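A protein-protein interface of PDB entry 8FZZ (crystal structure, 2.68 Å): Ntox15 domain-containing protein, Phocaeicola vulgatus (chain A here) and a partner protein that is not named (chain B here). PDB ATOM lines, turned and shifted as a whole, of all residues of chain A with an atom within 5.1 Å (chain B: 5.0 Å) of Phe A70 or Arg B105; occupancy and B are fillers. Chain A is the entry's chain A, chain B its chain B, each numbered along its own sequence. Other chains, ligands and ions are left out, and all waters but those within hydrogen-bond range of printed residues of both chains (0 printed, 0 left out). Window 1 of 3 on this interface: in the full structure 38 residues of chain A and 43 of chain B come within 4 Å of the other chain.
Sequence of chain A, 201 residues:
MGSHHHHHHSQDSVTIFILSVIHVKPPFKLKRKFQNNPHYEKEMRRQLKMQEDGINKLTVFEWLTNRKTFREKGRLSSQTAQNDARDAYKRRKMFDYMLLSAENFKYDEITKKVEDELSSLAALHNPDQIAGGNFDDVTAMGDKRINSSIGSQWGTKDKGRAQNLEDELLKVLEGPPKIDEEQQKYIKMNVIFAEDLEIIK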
ATOM      1  N   ASN A  66       6.898 -20.442   2.912  1.00  0.00           N
ATOM      2  CA  ASN A  66       5.918 -21.503   2.687  1.00  0.00           C
ATOM      3  C   ASN A  66       6.165 -22.730   3.561  1.00  0.00           C
ATOM      4  O   ASN A  66       5.209 -23.387   3.980  1.00  0.00           O
ATOM      5  CB  ASN A  66       5.915 -21.915   1.215  1.00  0.00           C
ATOM      6  CG  ASN A  66       5.307 -20.865   0.326  1.00  0.00           C
ATOM      7  OD1 ASN A  66       4.544 -20.020   0.790  1.00  0.00           O
ATOM      8  ND2 ASN A  66       5.652 -20.895  -0.958  1.00  0.00           N
ATOM      9  N   ARG A  67       7.419 -23.071   3.837  1.00  0.00           N
ATOM     10  CA  ARG A  67       7.672 -24.187   4.743  1.00  0.00           C
ATOM     11  C   ARG A  67       7.309 -23.830   6.185  1.00  0.00           C
ATOM     12  O   ARG A  67       6.776 -24.673   6.915  1.00  0.00           O
ATOM     13  CB  ARG A  67       9.130 -24.640   4.633  1.00  0.00           C
ATOM     14  CG  ARG A  67       9.411 -25.566   3.447  1.00  0.00           C
ATOM     15  CD  ARG A  67       9.037 -27.008   3.743  1.00  0.00           C
ATOM     16  NE  ARG A  67       9.406 -27.405   5.096  1.00  0.00           N
ATOM     17  CZ  ARG A  67       9.172 -28.603   5.624  1.00  0.00           C
ATOM     18  NH1 ARG A  67       8.579 -29.560   4.928  1.00  0.00           N
ATOM     19  NH2 ARG A  67       9.544 -28.844   6.881  1.00  0.00           N
ATOM     20  N   LYS A  68       7.585 -22.591   6.619  1.00  0.00           N
ATOM     21  CA  LYS A  68       7.083 -22.145   7.919  1.00  0.00           C
ATOM     22  C   LYS A  68       5.561 -22.218   7.972  1.00  0.00           C
ATOM     23  O   LYS A  68       4.987 -22.630   8.988  1.00  0.00           O
ATOM     24  CB  LYS A  68       7.541 -20.718   8.219  1.00  0.00           C
ATOM     25  CG  LYS A  68       8.685 -20.608   9.220  1.00  0.00           C
ATOM     26  CD  LYS A  68       8.374 -19.617  10.354  1.00  0.00           C
ATOM     27  CE  LYS A  68       9.473 -19.600  11.441  1.00  0.00           C
ATOM     28  NZ  LYS A  68       9.537 -20.843  12.292  1.00  0.00           N
ATOM     29  N   THR A  69       4.889 -21.809   6.890  1.00  0.00           N
ATOM     30  CA  THR A  69       3.429 -21.864   6.864  1.00  0.00           C
ATOM     31  C   THR A  69       2.937 -23.301   6.939  1.00  0.00           C
ATOM     32  O   THR A  69       1.930 -23.595   7.595  1.00  0.00           O
ATOM     33  CB  THR A  69       2.903 -21.157   5.608  1.00  0.00           C
ATOM     34  OG1 THR A  69       3.016 -19.743   5.779  1.00  0.00           O
ATOM     35  CG2 THR A  69       1.465 -21.491   5.333  1.00  0.00           C
ATOM     36  N   PHE A  70       3.647 -24.219   6.292  1.00  0.00           N
ATOM     37  CA  PHE A  70       3.231 -25.613   6.317  1.00  0.00           C
ATOM     38  C   PHE A  70       3.424 -26.222   7.701  1.00  0.00           C
ATOM     39  O   PHE A  70       2.536 -26.912   8.211  1.00  0.00           O
ATOM     40  CB  PHE A  70       4.006 -26.393   5.267  1.00  0.00           C
ATOM     41  CG  PHE A  70       3.847 -27.863   5.372  1.00  0.00           C
ATOM     42  CD1 PHE A  70       2.820 -28.500   4.708  1.00  0.00           C
ATOM     43  CD2 PHE A  70       4.730 -28.617   6.126  1.00  0.00           C
ATOM     44  CE1 PHE A  70       2.668 -29.862   4.798  1.00  0.00           C
ATOM     45  CE2 PHE A  70       4.586 -29.972   6.219  1.00  0.00           C
ATOM     46  CZ  PHE A  70       3.551 -30.600   5.553  1.00  0.00           C
ATOM     47  N   ARG A  71       4.579 -25.969   8.331  1.00  0.00           N
ATOM     48  CA  ARG A  71       4.895 -26.585   9.619  1.00  0.00           C
ATOM     49  C   ARG A  71       3.984 -26.121  10.751  1.00  0.00           C
ATOM     50  O   ARG A  71       3.832 -26.859  11.731  1.00  0.00           O
ATOM     51  CB  ARG A  71       6.356 -26.321   9.997  1.00  0.00           C
ATOM     52  CG  ARG A  71       7.361 -27.247   9.315  1.00  0.00           C
ATOM     53  CD  ARG A  71       8.805 -26.918   9.723  1.00  0.00           C
ATOM     54  NE  ARG A  71       8.897 -25.649  10.442  1.00  0.00           N
ATOM     55  CZ  ARG A  71       9.470 -24.543   9.974  1.00  0.00           C
ATOM     56  NH1 ARG A  71      10.048 -24.508   8.783  1.00  0.00           N
ATOM     57  NH2 ARG A  71       9.451 -23.438  10.717  1.00  0.00           N
ATOM     58  N   GLU A  72       3.362 -24.938  10.647  1.00  0.00           N
ATOM     59  CA  GLU A  72       2.437 -24.491  11.687  1.00  0.00           C
ATOM     60  C   GLU A  72       1.065 -25.152  11.549  1.00  0.00           C
ATOM     61  O   GLU A  72       0.039 -24.571  11.918  1.00  0.00           O
ATOM     62  CB  GLU A  72       2.312 -22.964  11.687  1.00  0.00           C
ATOM     63  CG  GLU A  72       2.212 -22.307  10.321  1.00  0.00           C
ATOM     64  CD  GLU A  72       1.389 -21.008  10.322  1.00  0.00           C
ATOM     65  OE1 GLU A  72       1.393 -20.300  11.357  1.00  0.00           O
ATOM     66  OE2 GLU A  72       0.776 -20.671   9.273  1.00  0.00           O
ATOM     67  N   LYS A  73       1.048 -26.382  11.039  1.00  0.00           N
ATOM     68  CA  LYS A  73      -0.157 -27.198  10.907  1.00  0.00           C
ATOM     69  C   LYS A  73       0.083 -28.504  11.656  1.00  0.00           C
ATOM     70  O   LYS A  73       0.950 -29.301  11.274  1.00  0.00           O
ATOM     71  CB  LYS A  73      -0.488 -27.456   9.437  1.00  0.00           C
ATOM     72  CG  LYS A  73      -0.957 -26.223   8.669  1.00  0.00           C
ATOM     73  CD  LYS A  73      -2.368 -26.431   8.137  1.00  0.00           C
ATOM     74  CE  LYS A  73      -2.765 -25.315   7.205  1.00  0.00           C
ATOM     75  NZ  LYS A  73      -1.721 -25.070   6.170  1.00  0.00           N
ATOM     76  N   THR B  81     -10.328 -38.105  -0.684  1.00  0.00           N
ATOM     77  CA  THR B  81     -10.983 -36.870  -1.092  1.00  0.00           C
ATOM     78  C   THR B  81     -10.486 -36.476  -2.470  1.00  0.00           C
ATOM     79  O   THR B  81      -9.616 -37.125  -3.050  1.00  0.00           O
ATOM     80  CB  THR B  81     -10.742 -35.723  -0.114  1.00  0.00           C
ATOM     81  OG1 THR B  81      -9.449 -35.143  -0.362  1.00  0.00           O
ATOM     82  CG2 THR B  81     -10.857 -36.191   1.331  1.00  0.00           C
ATOM     83  N   PHE B  83      -8.669 -34.061  -3.086  1.00  0.00           N
ATOM     84  CA  PHE B  83      -7.377 -33.419  -2.929  1.00  0.00           C
ATOM     85  C   PHE B  83      -6.258 -34.413  -2.636  1.00  0.00           C
ATOM     86  O   PHE B  83      -5.112 -33.990  -2.426  1.00  0.00           O
ATOM     87  CB  PHE B  83      -7.443 -32.377  -1.805  1.00  0.00           C
ATOM     88  CG  PHE B  83      -8.167 -31.107  -2.184  1.00  0.00           C
ATOM     89  CD1 PHE B  83      -7.567 -30.168  -3.009  1.00  0.00           C
ATOM     90  CD2 PHE B  83      -9.442 -30.845  -1.693  1.00  0.00           C
ATOM     91  CE1 PHE B  83      -8.219 -29.009  -3.346  1.00  0.00           C
ATOM     92  CE2 PHE B  83     -10.107 -29.682  -2.027  1.00  0.00           C
ATOM     93  CZ  PHE B  83      -9.495 -28.765  -2.855  1.00  0.00           C
ATOM     94  N   ASP B  85      -6.266 -36.592   0.021  1.00  0.00           N
ATOM     95  CA  ASP B  85      -6.335 -37.039   1.407  1.00  0.00           C
ATOM     96  C   ASP B  85      -6.887 -38.461   1.493  1.00  0.00           C
ATOM     97  O   ASP B  85      -7.676 -38.899   0.653  1.00  0.00           O
ATOM     98  CB  ASP B  85      -7.214 -36.092   2.214  1.00  0.00           C
ATOM     99  CG  ASP B  85      -6.922 -34.629   1.920  1.00  0.00           C
ATOM    100  OD1 ASP B  85      -5.721 -34.247   1.827  1.00  0.00           O
ATOM    101  OD2 ASP B  85      -7.906 -33.869   1.741  1.00  0.00           O
ATOM    102  N   PHE B 101      -7.824 -40.044   9.351  1.00  0.00           N
ATOM    103  CA  PHE B 101      -7.871 -39.145   8.202  1.00  0.00           C
ATOM    104  C   PHE B 101      -6.485 -38.531   8.063  1.00  0.00           C
ATOM    105  O   PHE B 101      -6.022 -37.815   8.961  1.00  0.00           O
ATOM    106  CB  PHE B 101      -8.940 -38.062   8.355  1.00  0.00           C
ATOM    107  CG  PHE B 101      -8.935 -37.053   7.235  1.00  0.00           C
ATOM    108  CD1 PHE B 101      -9.285 -37.432   5.946  1.00  0.00           C
ATOM    109  CD2 PHE B 101      -8.550 -35.737   7.462  1.00  0.00           C
ATOM    110  CE1 PHE B 101      -9.266 -36.516   4.908  1.00  0.00           C
ATOM    111  CE2 PHE B 101      -8.537 -34.814   6.429  1.00  0.00           C
ATOM    112  CZ  PHE B 101      -8.889 -35.208   5.150  1.00  0.00           C
ATOM    113  N   ASN B 103      -4.519 -35.937   6.068  1.00  0.00           N
ATOM    114  CA  ASN B 103      -4.569 -34.785   5.174  1.00  0.00           C
ATOM    115  C   ASN B 103      -3.260 -34.718   4.384  1.00  0.00           C
ATOM    116  O   ASN B 103      -2.213 -34.358   4.926  1.00  0.00           O
ATOM    117  CB  ASN B 103      -4.816 -33.515   5.979  1.00  0.00           C
ATOM    118  CG  ASN B 103      -5.330 -32.390   5.129  1.00  0.00           C
ATOM    119  OD1 ASN B 103      -4.831 -32.171   4.030  1.00  0.00           O
ATOM    120  ND2 ASN B 103      -6.342 -31.674   5.621  1.00  0.00           N
ATOM    121  N   ILE B 104      -3.308 -35.088   3.103  1.00  0.00           N
ATOM    122  CA  ILE B 104      -2.101 -35.126   2.292  1.00  0.00           C
ATOM    123  C   ILE B 104      -1.581 -33.730   1.989  1.00  0.00           C
ATOM    124  O   ILE B 104      -0.404 -33.578   1.653  1.00  0.00           O
ATOM    125  CB  ILE B 104      -2.363 -35.915   0.993  1.00  0.00           C
ATOM    126  CG1 ILE B 104      -1.160 -36.779   0.616  1.00  0.00           C
ATOM    127  CG2 ILE B 104      -2.747 -34.993  -0.154  1.00  0.00           C
ATOM    128  CD1 ILE B 104      -1.122 -38.091   1.385  1.00  0.00           C
ATOM    129  N   ARG B 105      -2.422 -32.697   2.097  1.00  0.00           N
ATOM    130  CA  ARG B 105      -1.966 -31.340   1.819  1.00  0.00           C
ATOM    131  C   ARG B 105      -1.189 -30.753   2.997  1.00  0.00           C
ATOM    132  O   ARG B 105      -0.150 -30.099   2.804  1.00  0.00           O
ATOM    133  CB  ARG B 105      -3.151 -30.437   1.508  1.00  0.00           C
ATOM    134  CG  ARG B 105      -3.710 -30.552   0.128  1.00  0.00           C
ATOM    135  CD  ARG B 105      -5.131 -30.047   0.142  1.00  0.00           C
ATOM    136  NE  ARG B 105      -6.014 -30.941   0.885  1.00  0.00           N
ATOM    137  CZ  ARG B 105      -6.946 -30.537   1.736  1.00  0.00           C
ATOM    138  NH1 ARG B 105      -7.126 -29.250   2.011  1.00  0.00           N
ATOM    139  NH2 ARG B 105      -7.713 -31.444   2.331  1.00  0.00           N
ATOM    140  N   TYR B 106      -1.688 -30.952   4.220  1.00  0.00           N
ATOM    141  CA  TYR B 106      -1.078 -30.391   5.417  1.00  0.00           C
ATOM    142  C   TYR B 106      -0.225 -31.383   6.175  1.00  0.00           C
ATOM    143  O   TYR B 106       0.350 -31.013   7.199  1.00  0.00           O
ATOM    144  CB  TYR B 106      -2.151 -29.841   6.355  1.00  0.00           C
ATOM    145  CG  TYR B 106      -3.012 -28.801   5.702  1.00  0.00           C
ATOM    146  CD1 TYR B 106      -2.492 -27.950   4.732  1.00  0.00           C
ATOM    147  CD2 TYR B 106      -4.348 -28.675   6.046  1.00  0.00           C
ATOM    148  CE1 TYR B 106      -3.288 -27.002   4.130  1.00  0.00           C
ATOM    149  CE2 TYR B 106      -5.156 -27.736   5.450  1.00  0.00           C
ATOM    150  CZ  TYR B 106      -4.624 -26.901   4.492  1.00  0.00           C
ATOM    151  OH  TYR B 106      -5.443 -25.964   3.906  1.00  0.00           O
ATOM    152  N   GLY B 107      -0.126 -32.619   5.700  1.00  0.00           N
ATOM    153  CA  GLY B 107       0.631 -33.647   6.400  1.00  0.00           C
ATOM    154  C   GLY B 107       0.187 -33.913   7.824  1.00  0.00           C
ATOM    155  O   GLY B 107       1.036 -34.083   8.707  1.00  0.00           O
ATOM    156  N   PHE B 134     -12.105 -31.924   7.678  1.00  0.00           N
ATOM    157  CA  PHE B 134     -11.403 -32.344   6.470  1.00  0.00           C
ATOM    158  C   PHE B 134     -10.859 -31.200   5.617  1.00  0.00           C
ATOM    159  O   PHE B 134     -10.111 -31.467   4.673  1.00  0.00           O
ATOM    160  CB  PHE B 134     -12.330 -33.222   5.619  1.00  0.00           C
ATOM    161  CG  PHE B 134     -12.989 -34.338   6.399  1.00  0.00           C
ATOM    162  CD1 PHE B 134     -12.226 -35.219   7.154  1.00  0.00           C
ATOM    163  CD2 PHE B 134     -14.364 -34.504   6.384  1.00  0.00           C
ATOM    164  CE1 PHE B 134     -12.833 -36.251   7.870  1.00  0.00           C
ATOM    165  CE2 PHE B 134     -14.963 -35.537   7.093  1.00  0.00           C
ATOM    166  CZ  PHE B 134     -14.197 -36.410   7.836  1.00  0.00           C
ATOM    167  N   ASP B 135     -11.208 -29.947   5.918  1.00  0.00           N
ATOM    168  CA  ASP B 135     -10.735 -28.775   5.171  1.00  0.00           C
ATOM    169  C   ASP B 135     -11.061 -28.879   3.678  1.00  0.00           C
ATOM    170  O   ASP B 135     -10.228 -28.607   2.812  1.00  0.00           O
ATOM    171  CB  ASP B 135      -9.236 -28.558   5.383  1.00  0.00           C
ATOM    172  CG  ASP B 135      -8.901 -28.220   6.808  1.00  0.00           C
ATOM    173  OD1 ASP B 135      -9.825 -27.777   7.528  1.00  0.00           O
ATOM    174  OD2 ASP B 135      -7.723 -28.386   7.210  1.00  0.00           O
ATOM    175  N   LEU B 136     -12.297 -29.263   3.374  1.00  0.00           N
ATOM    176  CA  LEU B 136     -12.728 -29.401   1.992  1.00  0.00           C
ATOM    177  C   LEU B 136     -13.708 -28.303   1.553  1.00  0.00           C
ATOM    178  O   LEU B 136     -14.411 -28.470   0.546  1.00  0.00           O
ATOM    179  CB  LEU B 136     -13.337 -30.786   1.801  1.00  0.00           C
ATOM    180  CG  LEU B 136     -12.368 -31.903   2.138  1.00  0.00           C
ATOM    181  CD1 LEU B 136     -13.077 -33.244   2.058  1.00  0.00           C
ATOM    182  CD2 LEU B 136     -11.199 -31.850   1.175  1.00  0.00           C
ATOM    183  N   TYR B 157      -1.073 -29.826  -5.628  1.00  0.00           N
ATOM    184  CA  TYR B 157      -0.302 -28.590  -5.609  1.00  0.00           C
ATOM    185  C   TYR B 157       1.091 -28.861  -6.163  1.00  0.00           C
ATOM    186  O   TYR B 157       1.707 -29.885  -5.846  1.00  0.00           O
ATOM    187  CB  TYR B 157      -0.213 -28.026  -4.190  1.00  0.00           C
ATOM    188  CG  TYR B 157      -1.535 -27.494  -3.703  1.00  0.00           C
ATOM    189  CD1 TYR B 157      -2.436 -28.321  -3.049  1.00  0.00           C
ATOM    190  CD2 TYR B 157      -1.893 -26.169  -3.924  1.00  0.00           C
ATOM    191  CE1 TYR B 157      -3.641 -27.843  -2.618  1.00  0.00           C
ATOM    192  CE2 TYR B 157      -3.100 -25.679  -3.499  1.00  0.00           C
ATOM    193  CZ  TYR B 157      -3.977 -26.520  -2.851  1.00  0.00           C
ATOM    194  OH  TYR B 157      -5.198 -26.030  -2.430  1.00  0.00           O
ATOM    195  N   LEU B 161       2.445 -28.214  -0.748  1.00  0.00           N
ATOM    196  CA  LEU B 161       2.652 -27.378   0.427  1.00  0.00           C
ATOM    197  C   LEU B 161       3.835 -27.877   1.253  1.00  0.00           C
ATOM    198  O   LEU B 161       4.618 -27.072   1.770  1.00  0.00           O
ATOM    199  CB  LEU B 161       1.371 -27.320   1.260  1.00  0.00           C
ATOM    200  CG  LEU B 161       0.146 -27.060   0.374  1.00  0.00           C
ATOM    201  CD1 LEU B 161      -1.139 -26.906   1.178  1.00  0.00           C
ATOM    202  CD2 LEU B 161       0.359 -25.822  -0.481  1.00  0.00           C
ATOM    203  N   SER B 162       4.015 -29.199   1.351  1.00  0.00           N
ATOM    204  CA  SER B 162       5.116 -29.718   2.159  1.00  0.00           C
ATOM    205  C   SER B 162       6.472 -29.384   1.551  1.00  0.00           C
ATOM    206  O   SER B 162       7.467 -29.298   2.276  1.00  0.00           O
ATOM    207  CB  SER B 162       4.977 -31.232   2.356  1.00  0.00           C
ATOM    208  OG  SER B 162       5.556 -31.956   1.286  1.00  0.00           O
ATOM    209  N   ILE B 188       6.785 -36.261   3.522  1.00  0.00           N
ATOM    210  CA  ILE B 188       6.538 -36.074   4.942  1.00  0.00           C
ATOM    211  C   ILE B 188       6.843 -37.386   5.652  1.00  0.00           C
ATOM    212  O   ILE B 188       6.434 -38.463   5.205  1.00  0.00           O
ATOM    213  CB  ILE B 188       5.087 -35.621   5.177  1.00  0.00           C
ATOM    214  CG1 ILE B 188       5.002 -34.103   5.126  1.00  0.00           C
ATOM    215  CG2 ILE B 188       4.554 -36.113   6.507  1.00  0.00           C
ATOM    216  CD1 ILE B 188       5.565 -33.430   6.366  1.00  0.00           C
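Phe A70 touches five residues of chain B.
Arg B105 touches just one residue of chain A: Phe A70 (3.5 Å).
Of the printed residues of chain A, Leu B161 touches Phe A70 (3.6 Å).
Printed residues of chain A within 4 Å of Tyr B106: Phe A70 and Lys A73.
Printed residues of chain A within 4 Å of Ile B188: Phe A70 (3.6 Å).
Printed residues of chain A within 4 Å of Ser B162: Arg A67 (2.9 Å) and Phe A70 (3.6 Å).
Ile B104 touches none of the printed residues of chain A.
Phe B83 touches none of the printed residues of chain A.
The nearest residue of chain B that does not touch Phe A70 is Gly B107 (4.03 Å).
The nearest printed residue of chain A that does not touch Arg B105 is Lys A73 (6.3 Å).
Among the printed residues, pairs that only touch across the chains: Lys A73 with Tyr B106, Phe A70 with Arg B105, Phe A70 with Tyr B106, Phe A70 with Ser B162, Phe A70 with Ile B188 and Phe A70 with Leu B161.
NH1 of Arg A67 sits at hydrogen-bond distance from O of Ser B162, at 2.9 Å.
Hydrophobic or aromatic side chains of chain B that line the printed part of chain A: Tyr B106, Leu B161 and Ile B188.
Of the 8 printed residues of chain A, 3 touch a printed residue of chain B.
Printed residues of chain A that touch a printed residue of chain B: Arg A67, Phe A70 and Lys A73.
Hydrophobic or aromatic side chains of chain A that line the printed part of chain B: Phe A70.
Among the printed residues, 7 pairs touch across the chains.
Among the printed residues, no Asp or Glu carboxylate lies within 4 Å of a Lys or Arg side-chain nitrogen of the other chain.
N of Tyr B106 is in hydrogen-bond range of OD1 of Asn B103, 3.4 Å away.
The guanidinium group of Arg B105 lies within hydrogen-bond range of the backbone carbonyl oxygen of Asp B135 (3.3 Å).
The backbone carbonyl oxygen (O) of Phe B134 is in hydrogen-bond range of the guanidinium group (NH2) of Arg B105, 3.4 Å away.
The side-chain amide oxygen (OD1) of Asn B103 lies within hydrogen-bond range of the backbone NH (N) of Arg B105 (3.1 Å).
OD2 of Asp B85 is in salt-bridge range of NH2 of Arg B105, 2.5 Å away.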
